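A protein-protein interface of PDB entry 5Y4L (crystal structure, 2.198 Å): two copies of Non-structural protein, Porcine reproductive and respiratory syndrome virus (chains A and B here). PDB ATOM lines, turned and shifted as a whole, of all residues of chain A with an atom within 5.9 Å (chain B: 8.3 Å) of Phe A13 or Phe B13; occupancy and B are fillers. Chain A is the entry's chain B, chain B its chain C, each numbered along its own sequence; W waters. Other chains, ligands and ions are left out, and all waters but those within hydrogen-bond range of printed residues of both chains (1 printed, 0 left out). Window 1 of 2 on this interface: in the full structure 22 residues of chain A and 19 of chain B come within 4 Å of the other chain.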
ATOM      1  N   GLY A  11     -38.442  12.144   2.936  1.00  0.00           N
ATOM      2  CA  GLY A  11     -37.179  11.447   2.704  1.00  0.00           C
ATOM      3  C   GLY A  11     -36.468  11.042   3.987  1.00  0.00           C
ATOM      4  O   GLY A  11     -36.846  10.055   4.621  1.00  0.00           O
ATOM      5  N   ALA A  12     -35.434  11.797   4.362  1.00  0.00           N
ATOM      6  CA  ALA A  12     -34.715  11.616   5.635  1.00  0.00           C
ATOM      7  C   ALA A  12     -34.415  12.969   6.304  1.00  0.00           C
ATOM      8  O   ALA A  12     -35.052  13.329   7.305  1.00  0.00           O
ATOM      9  CB  ALA A  12     -33.425  10.832   5.419  1.00  0.00           C
ATOM     10  N   PHE A  13     -33.457  13.714   5.749  1.00  0.00           N
ATOM     11  CA  PHE A  13     -33.142  15.088   6.211  1.00  0.00           C
ATOM     12  C   PHE A  13     -33.637  16.176   5.225  1.00  0.00           C
ATOM     13  O   PHE A  13     -32.898  17.130   4.919  1.00  0.00           O
ATOM     14  CB  PHE A  13     -31.629  15.273   6.400  1.00  0.00           C
ATOM     15  CG  PHE A  13     -31.112  14.926   7.773  1.00  0.00           C
ATOM     16  CD1 PHE A  13     -31.952  14.908   8.881  1.00  0.00           C
ATOM     17  CD2 PHE A  13     -29.754  14.654   7.961  1.00  0.00           C
ATOM     18  CE1 PHE A  13     -31.449  14.595  10.160  1.00  0.00           C
ATOM     19  CE2 PHE A  13     -29.240  14.346   9.232  1.00  0.00           C
ATOM     20  CZ  PHE A  13     -30.090  14.318  10.332  1.00  0.00           C
ATOM     21  N   ARG A  14     -34.874  16.043   4.751  1.00  0.00           N
ATOM     22  CA  ARG A  14     -35.371  16.823   3.615  1.00  0.00           C
ATOM     23  C   ARG A  14     -35.955  18.184   4.010  1.00  0.00           C
ATOM     24  O   ARG A  14     -36.676  18.294   4.988  1.00  0.00           O
ATOM     25  CB  ARG A  14     -36.432  16.001   2.857  1.00  0.00           C
ATOM     26  CG  ARG A  14     -36.859  16.618   1.506  1.00  0.00           C
ATOM     27  CD  ARG A  14     -37.615  15.589   0.655  1.00  0.00           C
ATOM     28  NE  ARG A  14     -36.786  14.409   0.375  1.00  0.00           N
ATOM     29  CZ  ARG A  14     -36.998  13.582  -0.643  1.00  0.00           C
ATOM     30  NH1 ARG A  14     -38.006  13.820  -1.480  1.00  0.00           N
ATOM     31  NH2 ARG A  14     -36.202  12.537  -0.844  1.00  0.00           N
ATOM     32  N   THR A  15     -35.679  19.234   3.247  1.00  0.00           N
ATOM     33  CA  THR A  15     -36.325  20.509   3.571  1.00  0.00           C
ATOM     34  C   THR A  15     -37.827  20.393   3.324  1.00  0.00           C
ATOM     35  O   THR A  15     -38.281  19.537   2.548  1.00  0.00           O
ATOM     36  CB  THR A  15     -35.760  21.678   2.763  1.00  0.00           C
ATOM     37  OG1 THR A  15     -35.924  21.419   1.353  1.00  0.00           O
ATOM     38  CG2 THR A  15     -34.274  21.891   3.128  1.00  0.00           C
ATOM     39  N   VAL A 109     -35.269  19.472  -0.670  1.00  0.00           N
ATOM     40  CA  VAL A 109     -33.883  19.217  -0.996  1.00  0.00           C
ATOM     41  C   VAL A 109     -33.404  18.186   0.003  1.00  0.00           C
ATOM     42  O   VAL A 109     -33.619  18.332   1.207  1.00  0.00           O
ATOM     43  CB  VAL A 109     -33.003  20.502  -0.921  1.00  0.00           C
ATOM     44  CG1 VAL A 109     -31.568  20.185  -1.275  1.00  0.00           C
ATOM     45  CG2 VAL A 109     -33.553  21.607  -1.854  1.00  0.00           C
ATOM     46  N   GLU A 110     -32.763  17.142  -0.514  1.00  0.00           N
ATOM     47  CA  GLU A 110     -32.273  16.034   0.277  1.00  0.00           C
ATOM     48  C   GLU A 110     -30.758  15.915   0.071  1.00  0.00           C
ATOM     49  O   GLU A 110     -30.284  15.872  -1.078  1.00  0.00           O
ATOM     50  CB  GLU A 110     -32.974  14.739  -0.147  1.00  0.00           C
ATOM     51  CG  GLU A 110     -32.483  13.502   0.585  1.00  0.00           C
ATOM     52  CD  GLU A 110     -33.238  13.288   1.883  1.00  0.00           C
ATOM     53  OE1 GLU A 110     -32.593  12.926   2.885  1.00  0.00           O
ATOM     54  OE2 GLU A 110     -34.476  13.482   1.889  1.00  0.00           O
ATOM     55  N   PRO A 111     -29.992  15.855   1.171  1.00  0.00           N
ATOM     56  CA  PRO A 111     -28.533  15.785   1.049  1.00  0.00           C
ATOM     57  C   PRO A 111     -28.087  14.377   0.675  1.00  0.00           C
ATOM     58  O   PRO A 111     -28.856  13.443   0.852  1.00  0.00           O
ATOM     59  CB  PRO A 111     -28.046  16.150   2.456  1.00  0.00           C
ATOM     60  CG  PRO A 111     -29.124  15.581   3.360  1.00  0.00           C
ATOM     61  CD  PRO A 111     -30.442  15.707   2.568  1.00  0.00           C
ATOM     62  N   SER A 201     -20.082  11.392  13.182  1.00  0.00           N
ATOM     63  CA  SER A 201     -21.394  11.768  13.707  1.00  0.00           C
ATOM     64  C   SER A 201     -22.398  12.211  12.625  1.00  0.00           C
ATOM     65  O   SER A 201     -23.585  11.929  12.728  1.00  0.00           O
ATOM     66  CB  SER A 201     -21.244  12.882  14.742  1.00  0.00           C
ATOM     67  OG  SER A 201     -20.596  14.001  14.159  1.00  0.00           O
ATOM     68  N   ASP A 202     -21.936  12.928  11.609  1.00  0.00           N
ATOM     69  CA  ASP A 202     -22.872  13.395  10.591  1.00  0.00           C
ATOM     70  C   ASP A 202     -23.515  12.227   9.839  1.00  0.00           C
ATOM     71  O   ASP A 202     -24.691  12.287   9.461  1.00  0.00           O
ATOM     72  CB  ASP A 202     -22.181  14.328   9.603  1.00  0.00           C
ATOM     73  CG  ASP A 202     -21.951  15.710  10.177  1.00  0.00           C
ATOM     74  OD1 ASP A 202     -22.385  15.985  11.327  1.00  0.00           O
ATOM     75  OD2 ASP A 202     -21.334  16.527   9.469  1.00  0.00           O
ATOM     76  N   ALA A 205     -26.090  10.460  12.236  1.00  0.00           N
ATOM     77  CA  ALA A 205     -27.332  11.232  12.320  1.00  0.00           C
ATOM     78  C   ALA A 205     -28.208  11.032  11.079  1.00  0.00           C
ATOM     79  O   ALA A 205     -29.427  10.897  11.176  1.00  0.00           O
ATOM     80  CB  ALA A 205     -27.029  12.719  12.506  1.00  0.00           C
ATOM     81  N   LEU A 206     -27.578  11.032   9.914  1.00  0.00           N
ATOM     82  CA  LEU A 206     -28.314  10.895   8.659  1.00  0.00           C
ATOM     83  C   LEU A 206     -28.953   9.525   8.598  1.00  0.00           C
ATOM     84  O   LEU A 206     -30.122   9.402   8.279  1.00  0.00           O
ATOM     85  CB  LEU A 206     -27.398  11.099   7.449  1.00  0.00           C
ATOM     86  CG  LEU A 206     -27.999  10.876   6.047  1.00  0.00           C
ATOM     87  CD1 LEU A 206     -29.167  11.804   5.754  1.00  0.00           C
ATOM     88  CD2 LEU A 206     -26.931  11.012   4.958  1.00  0.00           C
ATOM     89  N   ALA A 209     -31.967   8.943  10.680  1.00  0.00           N
ATOM     90  CA  ALA A 209     -33.100   9.794  10.347  1.00  0.00           C
ATOM     91  C   ALA A 209     -34.027   9.161   9.315  1.00  0.00           C
ATOM     92  O   ALA A 209     -35.135   9.656   9.107  1.00  0.00           O
ATOM     93  CB  ALA A 209     -32.615  11.143   9.843  1.00  0.00           C
ATOM     94  N   ALA B  12     -32.362  15.357  17.505  1.00  0.00           N
ATOM     95  CA  ALA B  12     -32.880  15.338  16.131  1.00  0.00           C
ATOM     96  C   ALA B  12     -31.734  15.209  15.121  1.00  0.00           C
ATOM     97  O   ALA B  12     -31.590  14.187  14.441  1.00  0.00           O
ATOM     98  CB  ALA B  12     -33.702  16.595  15.855  1.00  0.00           C
ATOM     99  N   PHE B  13     -30.908  16.252  15.039  1.00  0.00           N
ATOM    100  CA  PHE B  13     -29.641  16.142  14.337  1.00  0.00           C
ATOM    101  C   PHE B  13     -28.548  15.668  15.303  1.00  0.00           C
ATOM    102  O   PHE B  13     -27.375  15.642  14.953  1.00  0.00           O
ATOM    103  CB  PHE B  13     -29.254  17.472  13.699  1.00  0.00           C
ATOM    104  CG  PHE B  13     -29.641  17.591  12.245  1.00  0.00           C
ATOM    105  CD1 PHE B  13     -30.953  17.874  11.880  1.00  0.00           C
ATOM    106  CD2 PHE B  13     -28.691  17.443  11.243  1.00  0.00           C
ATOM    107  CE1 PHE B  13     -31.316  18.003  10.530  1.00  0.00           C
ATOM    108  CE2 PHE B  13     -29.039  17.575   9.893  1.00  0.00           C
ATOM    109  CZ  PHE B  13     -30.353  17.851   9.536  1.00  0.00           C
ATOM    110  N   ARG B  14     -28.944  15.297  16.518  1.00  0.00           N
ATOM    111  CA  ARG B  14     -28.017  14.715  17.494  1.00  0.00           C
ATOM    112  C   ARG B  14     -27.905  13.202  17.305  1.00  0.00           C
ATOM    113  O   ARG B  14     -28.922  12.534  17.106  1.00  0.00           O
ATOM    114  CB  ARG B  14     -28.480  15.035  18.918  1.00  0.00           C
ATOM    115  CG  ARG B  14     -27.526  14.577  20.022  1.00  0.00           C
ATOM    116  CD  ARG B  14     -27.945  15.159  21.368  1.00  0.00           C
ATOM    117  NE  ARG B  14     -28.028  16.619  21.341  1.00  0.00           N
ATOM    118  CZ  ARG B  14     -27.841  17.408  22.399  1.00  0.00           C
ATOM    119  NH1 ARG B  14     -27.551  16.880  23.597  1.00  0.00           N
ATOM    120  NH2 ARG B  14     -27.947  18.728  22.264  1.00  0.00           N
ATOM    121  N   THR B  15     -26.683  12.662  17.356  1.00  0.00           N
ATOM    122  CA  THR B  15     -26.504  11.208  17.304  1.00  0.00           C
ATOM    123  C   THR B  15     -27.225  10.571  18.493  1.00  0.00           C
ATOM    124  O   THR B  15     -27.560  11.254  19.461  1.00  0.00           O
ATOM    125  CB  THR B  15     -25.005  10.783  17.286  1.00  0.00           C
ATOM    126  OG1 THR B  15     -24.328  11.272  18.447  1.00  0.00           O
ATOM    127  CG2 THR B  15     -24.311  11.318  16.038  1.00  0.00           C
ATOM    128  N   GLN B  16     -27.526   9.284  18.397  1.00  0.00           N
ATOM    129  CA  GLN B  16     -28.244   8.600  19.471  1.00  0.00           C
ATOM    130  C   GLN B  16     -27.298   8.344  20.643  1.00  0.00           C
ATOM    131  O   GLN B  16     -27.687   8.456  21.797  1.00  0.00           O
ATOM    132  CB  GLN B  16     -28.857   7.287  18.970  1.00  0.00           C
ATOM    133  CG  GLN B  16     -30.145   7.464  18.145  1.00  0.00           C
ATOM    134  CD  GLN B  16     -30.493   6.229  17.323  1.00  0.00           C
ATOM    135  OE1 GLN B  16     -29.617   5.422  16.990  1.00  0.00           O
ATOM    136  NE2 GLN B  16     -31.775   6.072  16.999  1.00  0.00           N
ATOM    137  N   ARG B 100     -17.800  25.327  10.850  1.00  0.00           N
ATOM    138  CA  ARG B 100     -18.656  24.274  11.399  1.00  0.00           C
ATOM    139  C   ARG B 100     -17.907  23.479  12.469  1.00  0.00           C
ATOM    140  O   ARG B 100     -16.689  23.295  12.388  1.00  0.00           O
ATOM    141  CB  ARG B 100     -19.142  23.342  10.300  1.00  0.00           C
ATOM    142  CG  ARG B 100     -20.098  24.023   9.347  1.00  0.00           C
ATOM    143  CD  ARG B 100     -21.487  24.176   9.977  1.00  0.00           C
ATOM    144  NE  ARG B 100     -22.184  22.896  10.026  1.00  0.00           N
ATOM    145  CZ  ARG B 100     -22.708  22.302   8.957  1.00  0.00           C
ATOM    146  NH1 ARG B 100     -22.589  22.874   7.764  1.00  0.00           N
ATOM    147  NH2 ARG B 100     -23.335  21.137   9.069  1.00  0.00           N
ATOM    148  N   TYR B 102     -18.502  20.607  16.186  1.00  0.00           N
ATOM    149  CA  TYR B 102     -19.332  19.611  16.847  1.00  0.00           C
ATOM    150  C   TYR B 102     -19.283  19.742  18.352  1.00  0.00           C
ATOM    151  O   TYR B 102     -18.222  19.943  18.929  1.00  0.00           O
ATOM    152  CB  TYR B 102     -18.908  18.209  16.427  1.00  0.00           C
ATOM    153  CG  TYR B 102     -19.156  18.013  14.975  1.00  0.00           C
ATOM    154  CD1 TYR B 102     -20.402  17.624  14.511  1.00  0.00           C
ATOM    155  CD2 TYR B 102     -18.174  18.275  14.061  1.00  0.00           C
ATOM    156  CE1 TYR B 102     -20.628  17.477  13.205  1.00  0.00           C
ATOM    157  CE2 TYR B 102     -18.396  18.123  12.751  1.00  0.00           C
ATOM    158  CZ  TYR B 102     -19.618  17.718  12.321  1.00  0.00           C
ATOM    159  OH  TYR B 102     -19.822  17.578  10.959  1.00  0.00           O
ATOM    160  N   TRP B 103     -20.461  19.646  18.953  1.00  0.00           N
ATOM    161  CA  TRP B 103     -20.654  19.659  20.390  1.00  0.00           C
ATOM    162  C   TRP B 103     -20.752  18.210  20.870  1.00  0.00           C
ATOM    163  O   TRP B 103     -21.756  17.519  20.597  1.00  0.00           O
ATOM    164  CB  TRP B 103     -21.927  20.421  20.758  1.00  0.00           C
ATOM    165  CG  TRP B 103     -21.834  21.944  20.874  1.00  0.00           C
ATOM    166  CD1 TRP B 103     -22.075  22.691  21.992  1.00  0.00           C
ATOM    167  CD2 TRP B 103     -21.518  22.881  19.833  1.00  0.00           C
ATOM    168  NE1 TRP B 103     -21.929  24.032  21.720  1.00  0.00           N
ATOM    169  CE2 TRP B 103     -21.579  24.176  20.403  1.00  0.00           C
ATOM    170  CE3 TRP B 103     -21.203  22.754  18.473  1.00  0.00           C
ATOM    171  CZ2 TRP B 103     -21.339  25.337  19.658  1.00  0.00           C
ATOM    172  CZ3 TRP B 103     -20.966  23.916  17.728  1.00  0.00           C
ATOM    173  CH2 TRP B 103     -21.029  25.187  18.326  1.00  0.00           C
ATOM    174  N   GLY B 108     -25.076  12.701  23.052  1.00  0.00           N
ATOM    175  CA  GLY B 108     -24.794  12.593  21.629  1.00  0.00           C
ATOM    176  C   GLY B 108     -24.148  13.819  21.012  1.00  0.00           C
ATOM    177  O   GLY B 108     -24.193  14.908  21.584  1.00  0.00           O
ATOM    178  N   VAL B 109     -23.542  13.634  19.844  1.00  0.00           N
ATOM    179  CA  VAL B 109     -22.926  14.734  19.122  1.00  0.00           C
ATOM    180  C   VAL B 109     -23.932  15.578  18.321  1.00  0.00           C
ATOM    181  O   VAL B 109     -24.634  15.067  17.448  1.00  0.00           O
ATOM    182  CB  VAL B 109     -21.855  14.230  18.167  1.00  0.00           C
ATOM    183  CG1 VAL B 109     -21.170  15.417  17.446  1.00  0.00           C
ATOM    184  CG2 VAL B 109     -20.844  13.379  18.929  1.00  0.00           C
ATOM    185  N   GLU B 110     -23.963  16.875  18.625  1.00  0.00           N
ATOM    186  CA  GLU B 110     -24.791  17.878  17.936  1.00  0.00           C
ATOM    187  C   GLU B 110     -23.912  18.791  17.064  1.00  0.00           C
ATOM    188  O   GLU B 110     -22.872  19.280  17.540  1.00  0.00           O
ATOM    189  CB  GLU B 110     -25.550  18.715  18.966  1.00  0.00           C
ATOM    190  CG  GLU B 110     -26.504  19.744  18.402  1.00  0.00           C
ATOM    191  CD  GLU B 110     -27.911  19.175  18.194  1.00  0.00           C
ATOM    192  OE1 GLU B 110     -28.563  19.552  17.203  1.00  0.00           O
ATOM    193  OE2 GLU B 110     -28.358  18.352  19.029  1.00  0.00           O
ATOM    194  N   PRO B 111     -24.307  19.020  15.788  1.00  0.00           N
ATOM    195  CA  PRO B 111     -23.536  19.921  14.914  1.00  0.00           C
ATOM    196  C   PRO B 111     -23.884  21.392  15.170  1.00  0.00           C
ATOM    197  O   PRO B 111     -24.990  21.697  15.631  1.00  0.00           O
ATOM    198  CB  PRO B 111     -23.972  19.496  13.505  1.00  0.00           C
ATOM    199  CG  PRO B 111     -25.421  19.127  13.694  1.00  0.00           C
ATOM    200  CD  PRO B 111     -25.501  18.487  15.096  1.00  0.00           C
ATOM    201  N   GLY B 112     -22.953  22.294  14.888  1.00  0.00           N
ATOM    202  CA  GLY B 112     -23.241  23.704  15.062  1.00  0.00           C
ATOM    203  C   GLY B 112     -22.263  24.614  14.355  1.00  0.00           C
ATOM    204  O   GLY B 112     -21.504  24.177  13.493  1.00  0.00           O
ATOM    205  N   PHE B 122     -28.115  23.798  18.724  1.00  0.00           N
ATOM    206  CA  PHE B 122     -29.264  23.521  19.587  1.00  0.00           C
ATOM    207  C   PHE B 122     -28.857  22.602  20.730  1.00  0.00           C
ATOM    208  O   PHE B 122     -28.641  21.399  20.545  1.00  0.00           O
ATOM    209  CB  PHE B 122     -30.424  22.914  18.796  1.00  0.00           C
ATOM    210  CG  PHE B 122     -31.012  23.852  17.816  1.00  0.00           C
ATOM    211  CD1 PHE B 122     -31.776  24.928  18.253  1.00  0.00           C
ATOM    212  CD2 PHE B 122     -30.794  23.682  16.465  1.00  0.00           C
ATOM    213  CE1 PHE B 122     -32.327  25.805  17.362  1.00  0.00           C
ATOM    214  CE2 PHE B 122     -31.342  24.564  15.555  1.00  0.00           C
ATOM    215  CZ  PHE B 122     -32.101  25.628  15.998  1.00  0.00           C
ATOM    216  N   PHE B 176     -23.410  27.120   5.887  1.00  0.00           N
ATOM    217  CA  PHE B 176     -24.192  25.948   5.468  1.00  0.00           C
ATOM    218  C   PHE B 176     -24.224  25.836   3.948  1.00  0.00           C
ATOM    219  O   PHE B 176     -24.361  26.826   3.250  1.00  0.00           O
ATOM    220  CB  PHE B 176     -25.615  26.024   6.041  1.00  0.00           C
ATOM    221  CG  PHE B 176     -25.663  25.919   7.545  1.00  0.00           C
ATOM    222  CD1 PHE B 176     -25.428  27.033   8.343  1.00  0.00           C
ATOM    223  CD2 PHE B 176     -25.902  24.684   8.169  1.00  0.00           C
ATOM    224  CE1 PHE B 176     -25.438  26.928   9.738  1.00  0.00           C
ATOM    225  CE2 PHE B 176     -25.909  24.573   9.573  1.00  0.00           C
ATOM    226  CZ  PHE B 176     -25.692  25.692  10.351  1.00  0.00           C
ATOM    227  N   SER B 201     -30.224  24.965   1.990  1.00  0.00           N
ATOM    228  CA  SER B 201     -31.027  23.812   2.418  1.00  0.00           C
ATOM    229  C   SER B 201     -30.495  23.148   3.695  1.00  0.00           C
ATOM    230  O   SER B 201     -31.294  22.789   4.556  1.00  0.00           O
ATOM    231  CB  SER B 201     -31.119  22.764   1.301  1.00  0.00           C
ATOM    232  OG  SER B 201     -29.844  22.222   0.958  1.00  0.00           O
ATOM    233  N   ASP B 202     -29.168  22.985   3.826  1.00  0.00           N
ATOM    234  CA  ASP B 202     -28.621  22.382   5.063  1.00  0.00           C
ATOM    235  C   ASP B 202     -29.071  23.176   6.290  1.00  0.00           C
ATOM    236  O   ASP B 202     -29.388  22.585   7.328  1.00  0.00           O
ATOM    237  CB  ASP B 202     -27.087  22.304   5.041  1.00  0.00           C
ATOM    238  CG  ASP B 202     -26.570  21.135   4.220  1.00  0.00           C
ATOM    239  OD1 ASP B 202     -27.386  20.388   3.645  1.00  0.00           O
ATOM    240  OD2 ASP B 202     -25.336  20.976   4.096  1.00  0.00           O
ATOM    241  N   LEU B 203     -29.115  24.505   6.176  1.00  0.00           N
ATOM    242  CA  LEU B 203     -29.529  25.317   7.323  1.00  0.00           C
ATOM    243  C   LEU B 203     -31.016  25.144   7.569  1.00  0.00           C
ATOM    244  O   LEU B 203     -31.438  24.934   8.710  1.00  0.00           O
ATOM    245  CB  LEU B 203     -29.170  26.806   7.131  1.00  0.00           C
ATOM    246  CG  LEU B 203     -29.661  27.824   8.190  1.00  0.00           C
ATOM    247  CD1 LEU B 203     -29.253  27.460   9.619  1.00  0.00           C
ATOM    248  CD2 LEU B 203     -29.202  29.264   7.884  1.00  0.00           C
ATOM    249  N   CYS B 204     -31.826  25.205   6.518  1.00  0.00           N
ATOM    250  CA  CYS B 204     -33.276  25.079   6.730  1.00  0.00           C
ATOM    251  C   CYS B 204     -33.626  23.717   7.306  1.00  0.00           C
ATOM    252  O   CYS B 204     -34.533  23.588   8.127  1.00  0.00           O
ATOM    253  CB  CYS B 204     -34.048  25.296   5.443  1.00  0.00           C
ATOM    254  SG  CYS B 204     -35.810  25.434   5.759  1.00  0.00           S
ATOM    255  N   ALA B 205     -32.906  22.685   6.895  1.00  0.00           N
ATOM    256  CA  ALA B 205     -33.168  21.378   7.492  1.00  0.00           C
ATOM    257  C   ALA B 205     -32.802  21.400   8.991  1.00  0.00           C
ATOM    258  O   ALA B 205     -33.547  20.882   9.830  1.00  0.00           O
ATOM    259  CB  ALA B 205     -32.422  20.311   6.773  1.00  0.00           C
ATOM    260  N   LEU B 206     -31.684  22.031   9.335  1.00  0.00           N
ATOM    261  CA  LEU B 206     -31.310  22.116  10.743  1.00  0.00           C
ATOM    262  C   LEU B 206     -32.345  22.905  11.557  1.00  0.00           C
ATOM    263  O   LEU B 206     -32.765  22.463  12.623  1.00  0.00           O
ATOM    264  CB  LEU B 206     -29.922  22.734  10.893  1.00  0.00           C
ATOM    265  CG  LEU B 206     -29.403  22.901  12.323  1.00  0.00           C
ATOM    266  CD1 LEU B 206     -29.351  21.578  13.076  1.00  0.00           C
ATOM    267  CD2 LEU B 206     -28.031  23.546  12.295  1.00  0.00           C
ATOM    268  N   LEU B 207     -32.777  24.053  11.046  1.00  0.00           N
ATOM    269  CA  LEU B 207     -33.718  24.908  11.769  1.00  0.00           C
ATOM    270  C   LEU B 207     -35.063  24.216  11.984  1.00  0.00           C
ATOM    271  O   LEU B 207     -35.700  24.391  13.009  1.00  0.00           O
ATOM    272  CB  LEU B 207     -33.941  26.222  11.015  1.00  0.00           C
ATOM    273  CG  LEU B 207     -32.774  27.196  10.907  1.00  0.00           C
ATOM    274  CD1 LEU B 207     -33.155  28.393  10.043  1.00  0.00           C
ATOM    275  CD2 LEU B 207     -32.350  27.631  12.321  1.00  0.00           C
ATOM    276  N   ALA B 208     -35.494  23.437  11.007  1.00  0.00           N
ATOM    277  CA  ALA B 208     -36.790  22.776  11.093  1.00  0.00           C
ATOM    278  C   ALA B 208     -36.748  21.563  12.024  1.00  0.00           C
ATOM    279  O   ALA B 208     -37.783  21.080  12.475  1.00  0.00           O
ATOM    280  CB  ALA B 208     -37.269  22.371   9.702  1.00  0.00           C
ATOM    281  N   ALA B 209     -35.545  21.082  12.315  1.00  0.00           N
ATOM    282  CA  ALA B 209     -35.363  19.957  13.235  1.00  0.00           C
ATOM    283  C   ALA B 209     -35.339  20.395  14.707  1.00  0.00           C
ATOM    284  O   ALA B 209     -35.142  19.576  15.604  1.00  0.00           O
ATOM    285  CB  ALA B 209     -34.089  19.211  12.895  1.00  0.00           C
ATOM    286  N   LYS B 210     -35.534  21.684  14.953  1.00  0.00           N
ATOM    287  CA  LYS B 210     -35.595  22.192  16.317  1.00  0.00           C
ATOM    288  C   LYS B 210     -37.049  22.297  16.789  1.00  0.00           C
ATOM    289  O   LYS B 210     -37.550  21.414  17.487  1.00  0.00           O
ATOM    290  CB  LYS B 210     -34.917  23.532  16.407  1.00  0.00           C
HETATM  291  O   HOH W   1     -30.990  11.194  13.026  1.00  0.00           O
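The side-chain hydroxyl (OH) of Tyr B102 sits close to the side-chain carboxylate (OD1) of Asp A202 (3.0 Å).
CE2 of Phe A13 touches CE2 of Phe B13, at 3.3 Å. Phe A13 touches Ala B205. Ser B201 touches Thr A15. Val A109 touches Ser B201. Ser A201 touches Thr B15. Tyr B102 touches Ser A201 (CE1 to OG, 3.6 Å). CG1 of Val B109 touches OG of Ser A201 (3.6 Å). CB of Ala A205 touches O of Phe B13 (3.8 Å).
Water W1 lies within hydrogen-bond range of O of Ala A205 (2.4 Å), O of Ala B12 (3.4 Å) and N of Ala A209 (3.4 Å).
Phe B13 touches its own counterpart, Phe A13. Phe A13 touches Ala B205, and with the chains exchanged Ala A205 touches Phe B13. Thr A15 touches Ser B201, and with the chains exchanged Ser A201 touches Thr B15. Val A109 touches Ser B201, and with the chains exchanged Ser A201 touches Val B109.
The side-chain carboxylate (OE1) of Glu A110 is in hydrogen-bond range of the backbone NH (N) of Phe A13 (3.1 Å). OG1 of Thr A15 lies within hydrogen-bond range of N of Val A109. The backbone NH (N) of Val B109 is in hydrogen-bond range of the side-chain hydroxyl (OG1) of Thr B15, at 2.9 Å.
Printed residues of chain A that touch a printed residue of chain B: Phe A13, Thr A15, Val A109, Ser A201, Asp A202 and Ala A205. Of the 25 printed residues of chain B, 6 touch a printed residue of chain A. Printed residues of chain B that touch a printed residue of chain A: Phe B13, Thr B15, Tyr B102, Val B109, Ser B201 and Ala B205. Hydrophobic or aromatic side chains of chain B within 4 Å of the printed part of chain A: Phe B13, Tyr B102, Val B109 and Ala B205. Along chain B the printed residues that touch a printed residue of chain A span positions 13 to 205.
Phe A13 touches just these residues of chain B: Phe B13 (3.3 Å) and Ala B205 (3.7 Å). Phe B13 touches two residues of chain A. Ala A12 touches none of the printed residues of chain B. Of the printed residues of chain B, Ala A205 touches Phe B13. Of the printed residues of chain B, Thr A15 touches Ser B201. Of the printed residues of chain A, Thr B15 touches Ser A201.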
